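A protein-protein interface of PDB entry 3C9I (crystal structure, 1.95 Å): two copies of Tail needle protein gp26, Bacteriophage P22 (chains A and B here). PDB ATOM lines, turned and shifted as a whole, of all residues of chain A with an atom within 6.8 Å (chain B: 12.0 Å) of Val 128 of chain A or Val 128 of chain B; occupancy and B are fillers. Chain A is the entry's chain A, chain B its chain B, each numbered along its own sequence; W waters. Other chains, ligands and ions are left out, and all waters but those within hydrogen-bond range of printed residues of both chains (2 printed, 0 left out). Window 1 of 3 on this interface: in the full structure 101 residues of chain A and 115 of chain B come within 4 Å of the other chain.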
ATOM      1  N   SER A 123       6.457 -25.084 -23.627  1.00  0.00           N
ATOM      2  CA  SER A 123       7.854 -24.751 -23.870  1.00  0.00           C
ATOM      3  C   SER A 123       8.742 -25.794 -23.189  1.00  0.00           C
ATOM      4  O   SER A 123       9.835 -26.104 -23.682  1.00  0.00           O
ATOM      5  CB  SER A 123       8.178 -23.340 -23.360  1.00  0.00           C
ATOM      6  OG  SER A 123       8.079 -23.271 -21.953  1.00  0.00           O
ATOM      7  N   LEU A 124       8.281 -26.346 -22.067  1.00  0.00           N
ATOM      8  CA  LEU A 124       9.060 -27.368 -21.370  1.00  0.00           C
ATOM      9  C   LEU A 124       9.208 -28.563 -22.308  1.00  0.00           C
ATOM     10  O   LEU A 124      10.293 -29.118 -22.465  1.00  0.00           O
ATOM     11  CB  LEU A 124       8.362 -27.823 -20.083  1.00  0.00           C
ATOM     12  CG  LEU A 124       8.571 -26.971 -18.830  1.00  0.00           C
ATOM     13  CD1 LEU A 124       7.632 -27.418 -17.691  1.00  0.00           C
ATOM     14  CD2 LEU A 124      10.007 -27.099 -18.405  1.00  0.00           C
ATOM     15  N   GLN A 125       8.104 -28.951 -22.945  1.00  0.00           N
ATOM     16  CA  GLN A 125       8.145 -30.086 -23.849  1.00  0.00           C
ATOM     17  C   GLN A 125       9.161 -29.886 -24.973  1.00  0.00           C
ATOM     18  O   GLN A 125       9.984 -30.767 -25.230  1.00  0.00           O
ATOM     19  CB  GLN A 125       6.751 -30.354 -24.411  1.00  0.00           C
ATOM     20  CG  GLN A 125       5.831 -31.014 -23.392  1.00  0.00           C
ATOM     21  CD  GLN A 125       4.412 -31.163 -23.883  1.00  0.00           C
ATOM     22  OE1 GLN A 125       3.572 -31.767 -23.217  1.00  0.00           O
ATOM     23  NE2 GLN A 125       4.131 -30.607 -25.054  1.00  0.00           N
ATOM     24  N   THR A 126       9.106 -28.729 -25.629  1.00  0.00           N
ATOM     25  CA  THR A 126      10.041 -28.438 -26.704  1.00  0.00           C
ATOM     26  C   THR A 126      11.474 -28.490 -26.174  1.00  0.00           C
ATOM     27  O   THR A 126      12.354 -29.084 -26.805  1.00  0.00           O
ATOM     28  CB  THR A 126       9.768 -27.047 -27.310  1.00  0.00           C
ATOM     29  OG1 THR A 126       8.445 -27.015 -27.857  1.00  0.00           O
ATOM     30  CG2 THR A 126      10.757 -26.744 -28.412  1.00  0.00           C
ATOM     31  N   ASN A 127      11.708 -27.892 -25.006  1.00  0.00           N
ATOM     32  CA  ASN A 127      13.044 -27.897 -24.408  1.00  0.00           C
ATOM     33  C   ASN A 127      13.532 -29.297 -24.047  1.00  0.00           C
ATOM     34  O   ASN A 127      14.686 -29.643 -24.303  1.00  0.00           O
ATOM     35  CB  ASN A 127      13.096 -27.017 -23.153  1.00  0.00           C
ATOM     36  CG  ASN A 127      13.146 -25.540 -23.479  1.00  0.00           C
ATOM     37  OD1 ASN A 127      13.895 -25.112 -24.351  1.00  0.00           O
ATOM     38  ND2 ASN A 127      12.353 -24.748 -22.765  1.00  0.00           N
ATOM     39  N   VAL A 128      12.679 -30.106 -23.433  1.00  0.00           N
ATOM     40  CA  VAL A 128      13.115 -31.444 -23.082  1.00  0.00           C
ATOM     41  C   VAL A 128      13.344 -32.272 -24.342  1.00  0.00           C
ATOM     42  O   VAL A 128      14.269 -33.082 -24.408  1.00  0.00           O
ATOM     43  CB  VAL A 128      12.102 -32.137 -22.172  1.00  0.00           C
ATOM     44  CG1 VAL A 128      12.381 -33.628 -22.125  1.00  0.00           C
ATOM     45  CG2 VAL A 128      12.203 -31.550 -20.775  1.00  0.00           C
ATOM     46  N   SER A 129      12.506 -32.046 -25.345  1.00  0.00           N
ATOM     47  CA  SER A 129      12.617 -32.753 -26.603  1.00  0.00           C
ATOM     48  C   SER A 129      13.983 -32.447 -27.227  1.00  0.00           C
ATOM     49  O   SER A 129      14.678 -33.343 -27.717  1.00  0.00           O
ATOM     50  CB  SER A 129      11.488 -32.303 -27.532  1.00  0.00           C
ATOM     51  OG  SER A 129      11.621 -32.895 -28.814  1.00  0.00           O
ATOM     52  N   ALA A 130      14.378 -31.180 -27.191  1.00  0.00           N
ATOM     53  CA  ALA A 130      15.658 -30.774 -27.759  1.00  0.00           C
ATOM     54  C   ALA A 130      16.789 -31.306 -26.905  1.00  0.00           C
ATOM     55  O   ALA A 130      17.813 -31.784 -27.404  1.00  0.00           O
ATOM     56  CB  ALA A 130      15.732 -29.259 -27.828  1.00  0.00           C
ATOM     57  N   LEU A 131      16.611 -31.205 -25.596  1.00  0.00           N
ATOM     58  CA  LEU A 131      17.622 -31.681 -24.668  1.00  0.00           C
ATOM     59  C   LEU A 131      17.827 -33.166 -24.921  1.00  0.00           C
ATOM     60  O   LEU A 131      18.935 -33.690 -24.788  1.00  0.00           O
ATOM     61  CB  LEU A 131      17.137 -31.428 -23.246  1.00  0.00           C
ATOM     62  CG  LEU A 131      18.142 -31.173 -22.134  1.00  0.00           C
ATOM     63  CD1 LEU A 131      19.327 -30.372 -22.655  1.00  0.00           C
ATOM     64  CD2 LEU A 131      17.430 -30.431 -21.014  1.00  0.00           C
ATOM     65  N   ASP A 132      16.747 -33.844 -25.300  1.00  0.00           N
ATOM     66  CA  ASP A 132      16.802 -35.269 -25.574  1.00  0.00           C
ATOM     67  C   ASP A 132      17.727 -35.533 -26.749  1.00  0.00           C
ATOM     68  O   ASP A 132      18.529 -36.463 -26.725  1.00  0.00           O
ATOM     69  CB  ASP A 132      15.410 -35.802 -25.898  1.00  0.00           C
ATOM     70  CG  ASP A 132      15.069 -37.044 -25.104  1.00  0.00           C
ATOM     71  OD1 ASP A 132      14.333 -36.925 -24.098  1.00  0.00           O
ATOM     72  OD2 ASP A 132      15.553 -38.136 -25.477  1.00  0.00           O
ATOM     73  N   GLY A 133      17.606 -34.706 -27.782  1.00  0.00           N
ATOM     74  CA  GLY A 133      18.437 -34.866 -28.953  1.00  0.00           C
ATOM     75  C   GLY A 133      19.896 -34.608 -28.633  1.00  0.00           C
ATOM     76  O   GLY A 133      20.776 -35.326 -29.097  1.00  0.00           O
ATOM     77  N   GLY B 119       2.979 -25.761  -8.989  1.00  0.00           N
ATOM     78  CA  GLY B 119       4.170 -26.051  -8.215  1.00  0.00           C
ATOM     79  C   GLY B 119       5.071 -27.016  -8.957  1.00  0.00           C
ATOM     80  O   GLY B 119       6.295 -26.847  -9.001  1.00  0.00           O
ATOM     81  N   GLU B 120       4.459 -28.036  -9.547  1.00  0.00           N
ATOM     82  CA  GLU B 120       5.198 -29.031 -10.299  1.00  0.00           C
ATOM     83  C   GLU B 120       5.873 -28.379 -11.497  1.00  0.00           C
ATOM     84  O   GLU B 120       6.995 -28.742 -11.850  1.00  0.00           O
ATOM     85  CB  GLU B 120       4.257 -30.142 -10.761  1.00  0.00           C
ATOM     86  CG  GLU B 120       3.611 -30.885  -9.611  1.00  0.00           C
ATOM     87  CD  GLU B 120       2.572 -31.884 -10.064  1.00  0.00           C
ATOM     88  OE1 GLU B 120       1.582 -31.458 -10.692  1.00  0.00           O
ATOM     89  OE2 GLU B 120       2.738 -33.089  -9.785  1.00  0.00           O
ATOM     90  N   ILE B 121       5.187 -27.418 -12.113  1.00  0.00           N
ATOM     91  CA  ILE B 121       5.737 -26.720 -13.271  1.00  0.00           C
ATOM     92  C   ILE B 121       6.968 -25.922 -12.865  1.00  0.00           C
ATOM     93  O   ILE B 121       7.995 -25.989 -13.525  1.00  0.00           O
ATOM     94  CB  ILE B 121       4.693 -25.756 -13.923  1.00  0.00           C
ATOM     95  CG1 ILE B 121       3.673 -26.556 -14.734  1.00  0.00           C
ATOM     96  CG2 ILE B 121       5.385 -24.774 -14.869  1.00  0.00           C
ATOM     97  CD1 ILE B 121       2.625 -25.683 -15.423  1.00  0.00           C
ATOM     98  N   ALA B 122       6.863 -25.182 -11.766  1.00  0.00           N
ATOM     99  CA  ALA B 122       7.977 -24.368 -11.292  1.00  0.00           C
ATOM    100  C   ALA B 122       9.246 -25.187 -11.093  1.00  0.00           C
ATOM    101  O   ALA B 122      10.331 -24.778 -11.518  1.00  0.00           O
ATOM    102  CB  ALA B 122       7.595 -23.671  -9.994  1.00  0.00           C
ATOM    103  N   SER B 123       9.115 -26.342 -10.447  1.00  0.00           N
ATOM    104  CA  SER B 123      10.264 -27.207 -10.204  1.00  0.00           C
ATOM    105  C   SER B 123      10.808 -27.810 -11.504  1.00  0.00           C
ATOM    106  O   SER B 123      12.025 -27.895 -11.676  1.00  0.00           O
ATOM    107  CB  SER B 123       9.898 -28.324  -9.215  1.00  0.00           C
ATOM    108  OG  SER B 123       9.033 -29.270  -9.807  1.00  0.00           O
ATOM    109  N   LEU B 124       9.918 -28.225 -12.411  1.00  0.00           N
ATOM    110  CA  LEU B 124      10.346 -28.794 -13.693  1.00  0.00           C
ATOM    111  C   LEU B 124      11.229 -27.792 -14.429  1.00  0.00           C
ATOM    112  O   LEU B 124      12.266 -28.156 -14.977  1.00  0.00           O
ATOM    113  CB  LEU B 124       9.144 -29.150 -14.576  1.00  0.00           C
ATOM    114  CG  LEU B 124       8.560 -30.562 -14.427  1.00  0.00           C
ATOM    115  CD1 LEU B 124       7.175 -30.635 -15.044  1.00  0.00           C
ATOM    116  CD2 LEU B 124       9.500 -31.565 -15.074  1.00  0.00           C
ATOM    117  N   GLN B 125      10.817 -26.530 -14.446  1.00  0.00           N
ATOM    118  CA  GLN B 125      11.613 -25.499 -15.115  1.00  0.00           C
ATOM    119  C   GLN B 125      12.988 -25.386 -14.460  1.00  0.00           C
ATOM    120  O   GLN B 125      13.994 -25.184 -15.133  1.00  0.00           O
ATOM    121  CB  GLN B 125      10.891 -24.155 -15.056  1.00  0.00           C
ATOM    122  CG  GLN B 125       9.520 -24.197 -15.711  1.00  0.00           C
ATOM    123  CD  GLN B 125       8.839 -22.845 -15.739  1.00  0.00           C
ATOM    124  OE1 GLN B 125       8.732 -22.172 -14.715  1.00  0.00           O
ATOM    125  NE2 GLN B 125       8.366 -22.443 -16.911  1.00  0.00           N
ATOM    126  N   THR B 126      13.013 -25.526 -13.138  1.00  0.00           N
ATOM    127  CA  THR B 126      14.250 -25.456 -12.367  1.00  0.00           C
ATOM    128  C   THR B 126      15.175 -26.616 -12.739  1.00  0.00           C
ATOM    129  O   THR B 126      16.383 -26.442 -12.899  1.00  0.00           O
ATOM    130  CB  THR B 126      13.960 -25.538 -10.852  1.00  0.00           C
ATOM    131  OG1 THR B 126      13.357 -24.316 -10.409  1.00  0.00           O
ATOM    132  CG2 THR B 126      15.248 -25.792 -10.068  1.00  0.00           C
ATOM    133  N   ASN B 127      14.598 -27.805 -12.867  1.00  0.00           N
ATOM    134  CA  ASN B 127      15.383 -28.974 -13.200  1.00  0.00           C
ATOM    135  C   ASN B 127      15.888 -28.936 -14.632  1.00  0.00           C
ATOM    136  O   ASN B 127      17.046 -29.271 -14.889  1.00  0.00           O
ATOM    137  CB  ASN B 127      14.573 -30.246 -12.953  1.00  0.00           C
ATOM    138  CG  ASN B 127      14.332 -30.498 -11.477  1.00  0.00           C
ATOM    139  OD1 ASN B 127      15.210 -30.256 -10.651  1.00  0.00           O
ATOM    140  ND2 ASN B 127      13.149 -30.998 -11.138  1.00  0.00           N
ATOM    141  N   VAL B 128      15.029 -28.522 -15.559  1.00  0.00           N
ATOM    142  CA  VAL B 128      15.423 -28.445 -16.958  1.00  0.00           C
ATOM    143  C   VAL B 128      16.510 -27.382 -17.133  1.00  0.00           C
ATOM    144  O   VAL B 128      17.476 -27.589 -17.871  1.00  0.00           O
ATOM    145  CB  VAL B 128      14.214 -28.120 -17.854  1.00  0.00           C
ATOM    146  CG1 VAL B 128      14.674 -27.715 -19.238  1.00  0.00           C
ATOM    147  CG2 VAL B 128      13.310 -29.343 -17.960  1.00  0.00           C
ATOM    148  N   SER B 129      16.368 -26.250 -16.449  1.00  0.00           N
ATOM    149  CA  SER B 129      17.371 -25.186 -16.551  1.00  0.00           C
ATOM    150  C   SER B 129      18.758 -25.711 -16.192  1.00  0.00           C
ATOM    151  O   SER B 129      19.713 -25.557 -16.952  1.00  0.00           O
ATOM    152  CB  SER B 129      17.021 -24.035 -15.612  1.00  0.00           C
ATOM    153  OG  SER B 129      15.833 -23.388 -16.012  1.00  0.00           O
ATOM    154  N   ALA B 130      18.859 -26.311 -15.012  1.00  0.00           N
ATOM    155  CA  ALA B 130      20.114 -26.850 -14.530  1.00  0.00           C
ATOM    156  C   ALA B 130      20.640 -27.920 -15.480  1.00  0.00           C
ATOM    157  O   ALA B 130      21.833 -27.962 -15.774  1.00  0.00           O
ATOM    158  CB  ALA B 130      19.931 -27.434 -13.128  1.00  0.00           C
ATOM    159  N   LEU B 131      19.747 -28.774 -15.969  1.00  0.00           N
ATOM    160  CA  LEU B 131      20.151 -29.842 -16.876  1.00  0.00           C
ATOM    161  C   LEU B 131      20.792 -29.250 -18.121  1.00  0.00           C
ATOM    162  O   LEU B 131      21.820 -29.740 -18.592  1.00  0.00           O
ATOM    163  CB  LEU B 131      18.943 -30.684 -17.285  1.00  0.00           C
ATOM    164  CG  LEU B 131      19.260 -32.116 -17.718  1.00  0.00           C
ATOM    165  CD1 LEU B 131      19.827 -32.890 -16.537  1.00  0.00           C
ATOM    166  CD2 LEU B 131      17.998 -32.785 -18.227  1.00  0.00           C
ATOM    167  N   ASP B 132      20.167 -28.210 -18.662  1.00  0.00           N
ATOM    168  CA  ASP B 132      20.694 -27.549 -19.845  1.00  0.00           C
ATOM    169  C   ASP B 132      22.145 -27.104 -19.621  1.00  0.00           C
ATOM    170  O   ASP B 132      22.988 -27.277 -20.493  1.00  0.00           O
ATOM    171  CB  ASP B 132      19.827 -26.339 -20.192  1.00  0.00           C
ATOM    172  CG  ASP B 132      18.568 -26.721 -20.954  1.00  0.00           C
ATOM    173  OD1 ASP B 132      17.507 -26.108 -20.708  1.00  0.00           O
ATOM    174  OD2 ASP B 132      18.642 -27.626 -21.812  1.00  0.00           O
ATOM    175  N   GLY B 133      22.424 -26.534 -18.454  1.00  0.00           N
ATOM    176  CA  GLY B 133      23.772 -26.074 -18.149  1.00  0.00           C
ATOM    177  C   GLY B 133      24.798 -27.193 -18.097  1.00  0.00           C
ATOM    178  O   GLY B 133      25.942 -27.022 -18.501  1.00  0.00           O
ATOM    179  N   ARG B 134      24.385 -28.348 -17.594  1.00  0.00           N
ATOM    180  CA  ARG B 134      25.272 -29.490 -17.509  1.00  0.00           C
ATOM    181  C   ARG B 134      25.513 -30.084 -18.895  1.00  0.00           C
ATOM    182  O   ARG B 134      26.621 -30.538 -19.198  1.00  0.00           O
ATOM    183  CB  ARG B 134      24.675 -30.550 -16.579  1.00  0.00           C
ATOM    184  CG  ARG B 134      24.833 -30.237 -15.099  1.00  0.00           C
ATOM    185  CD  ARG B 134      23.955 -31.140 -14.242  1.00  0.00           C
ATOM    186  NE  ARG B 134      24.384 -32.534 -14.272  1.00  0.00           N
ATOM    187  CZ  ARG B 134      23.637 -33.544 -13.839  1.00  0.00           C
ATOM    188  NH1 ARG B 134      22.432 -33.307 -13.352  1.00  0.00           N
ATOM    189  NH2 ARG B 134      24.094 -34.790 -13.882  1.00  0.00           N
ATOM    190  N   VAL B 135      24.485 -30.088 -19.738  1.00  0.00           N
ATOM    191  CA  VAL B 135      24.644 -30.645 -21.079  1.00  0.00           C
ATOM    192  C   VAL B 135      25.629 -29.787 -21.865  1.00  0.00           C
ATOM    193  O   VAL B 135      26.547 -30.304 -22.494  1.00  0.00           O
ATOM    194  CB  VAL B 135      23.293 -30.725 -21.820  1.00  0.00           C
ATOM    195  CG1 VAL B 135      23.510 -31.131 -23.271  1.00  0.00           C
ATOM    196  CG2 VAL B 135      22.397 -31.746 -21.137  1.00  0.00           C
ATOM    197  N   THR B 136      25.445 -28.473 -21.799  1.00  0.00           N
ATOM    198  CA  THR B 136      26.331 -27.545 -22.502  1.00  0.00           C
ATOM    199  C   THR B 136      27.778 -27.780 -22.088  1.00  0.00           C
ATOM    200  O   THR B 136      28.678 -27.823 -22.923  1.00  0.00           O
ATOM    201  CB  THR B 136      25.945 -26.076 -22.203  1.00  0.00           C
ATOM    202  OG1 THR B 136      24.630 -25.822 -22.707  1.00  0.00           O
ATOM    203  CG2 THR B 136      26.926 -25.105 -22.863  1.00  0.00           C
ATOM    204  N   THR B 137      27.988 -27.956 -20.790  1.00  0.00           N
ATOM    205  CA  THR B 137      29.317 -28.186 -20.243  1.00  0.00           C
ATOM    206  C   THR B 137      29.897 -29.533 -20.698  1.00  0.00           C
ATOM    207  O   THR B 137      31.052 -29.608 -21.104  1.00  0.00           O
ATOM    208  CB  THR B 137      29.271 -28.113 -18.700  1.00  0.00           C
ATOM    209  OG1 THR B 137      28.953 -26.777 -18.291  1.00  0.00           O
ATOM    210  CG2 THR B 137      30.593 -28.522 -18.097  1.00  0.00           C
ATOM    211  N   GLU B 139      29.097 -31.220 -23.323  1.00  0.00           N
ATOM    212  CA  GLU B 139      29.280 -31.060 -24.764  1.00  0.00           C
ATOM    213  C   GLU B 139      30.596 -30.366 -25.106  1.00  0.00           C
ATOM    214  O   GLU B 139      31.241 -30.705 -26.093  1.00  0.00           O
ATOM    215  CB  GLU B 139      28.129 -30.246 -25.356  1.00  0.00           C
ATOM    216  CG  GLU B 139      26.912 -31.053 -25.803  1.00  0.00           C
ATOM    217  CD  GLU B 139      25.688 -30.171 -26.079  1.00  0.00           C
ATOM    218  OE1 GLU B 139      24.794 -30.602 -26.850  1.00  0.00           O
ATOM    219  OE2 GLU B 139      25.618 -29.051 -25.516  1.00  0.00           O
HETATM  220  O   HOH W   1      16.566 -27.387 -24.486  1.00  0.00           O
HETATM  221  O   HOH W   2       8.444 -23.464 -19.322  1.00  0.00           O
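The backbone carbonyl oxygen of Gln 125 of chain B sits at hydrogen-bond distance from the side-chain hydroxyl of Ser 129 of chain B (2.7 Å).
The side-chain hydroxyl of Thr 136 of chain B is in hydrogen-bond range of the backbone carbonyl oxygen of Asp 132 of chain B (3.1 Å).
Leu 124 of chain A touches Leu 124 of chain B.
Gln 125 of chain B touches Leu 124 of chain A (CG to CD2, 3.99 Å).
Val 128 of chain B touches Val 128 of chain A (CG2 to CG2, 3.7 Å).
Leu 131 of chain B touches Leu 131 of chain A (CD2 to CD2, 3.7 Å).
Leu 131 of chain A touches Asp 132 of chain B (CD1 to OD2, 3.0 Å).
CD1 of Leu 131 of chain A touches CG2 of Val 135 of chain B, at 3.7 Å.
Val 128 of chain A touches one residue of chain B.
Of the printed residues of chain A, Val 128 of chain B touches Val 128 (3.7 Å).
No residue of chain B comes within 4 Å of Thr 126 of chain A.
No residue of chain B comes within 4 Å of Asn 127 of chain A.
No residue of chain B comes within 4 Å of Ser 129 of chain A.
Of the printed residues of chain A, Asp 132 of chain B touches Leu 131.
Of the printed residues of chain A, Gln 125 of chain B touches Leu 124.
Printed residues of chain B within 4 Å of Leu 124 of chain A: Leu 124 and Gln 125.
Printed residues of chain A within 4 Å of Leu 124 of chain B: Leu 124.
Printed residues of chain A within 4 Å of Val 135 of chain B: Leu 131 (3.7 Å).
The nearest printed residue of chain A that does not touch Val 128 of chain B is Leu 124 of chain A (4.02 Å).
Of the 20 printed residues of chain B, 6 touch a printed residue of chain A.
Of the 11 printed residues of chain A, 3 touch a printed residue of chain B.
Hydrophobic or aromatic side chains of chain A that line the printed part of chain B: Leu 124, Val 128 and Leu 131.
Leu 124 of chain B touches its own counterpart, Leu 124 of chain A.
Leu 124 of chain A touches Gln 125 of chain B, but with the chains exchanged Gln 125 of chain A does not touch Leu 124 of chain B (8.1 Å).
Val 128 of chain A touches its own counterpart, Val 128 of chain B.
Leu 131 of chain A touches Asp 132 of chain B, but with the chains exchanged Asp 132 of chain A does not touch Leu 131 of chain B (7.3 Å).
Of the 6 pairs that touch across the chains among the printed residues, 3 have their exchanged pair printed and touching as well.
Water W2 bridges NE2 of Gln 125 of chain B (2.6 Å) and OG of Ser 123 of chain A (2.7 Å).
Water W1 bridges the backbone carbonyl oxygen of Asn 127 of chain A and the side-chain carboxylate of Asp 132 of chain B.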
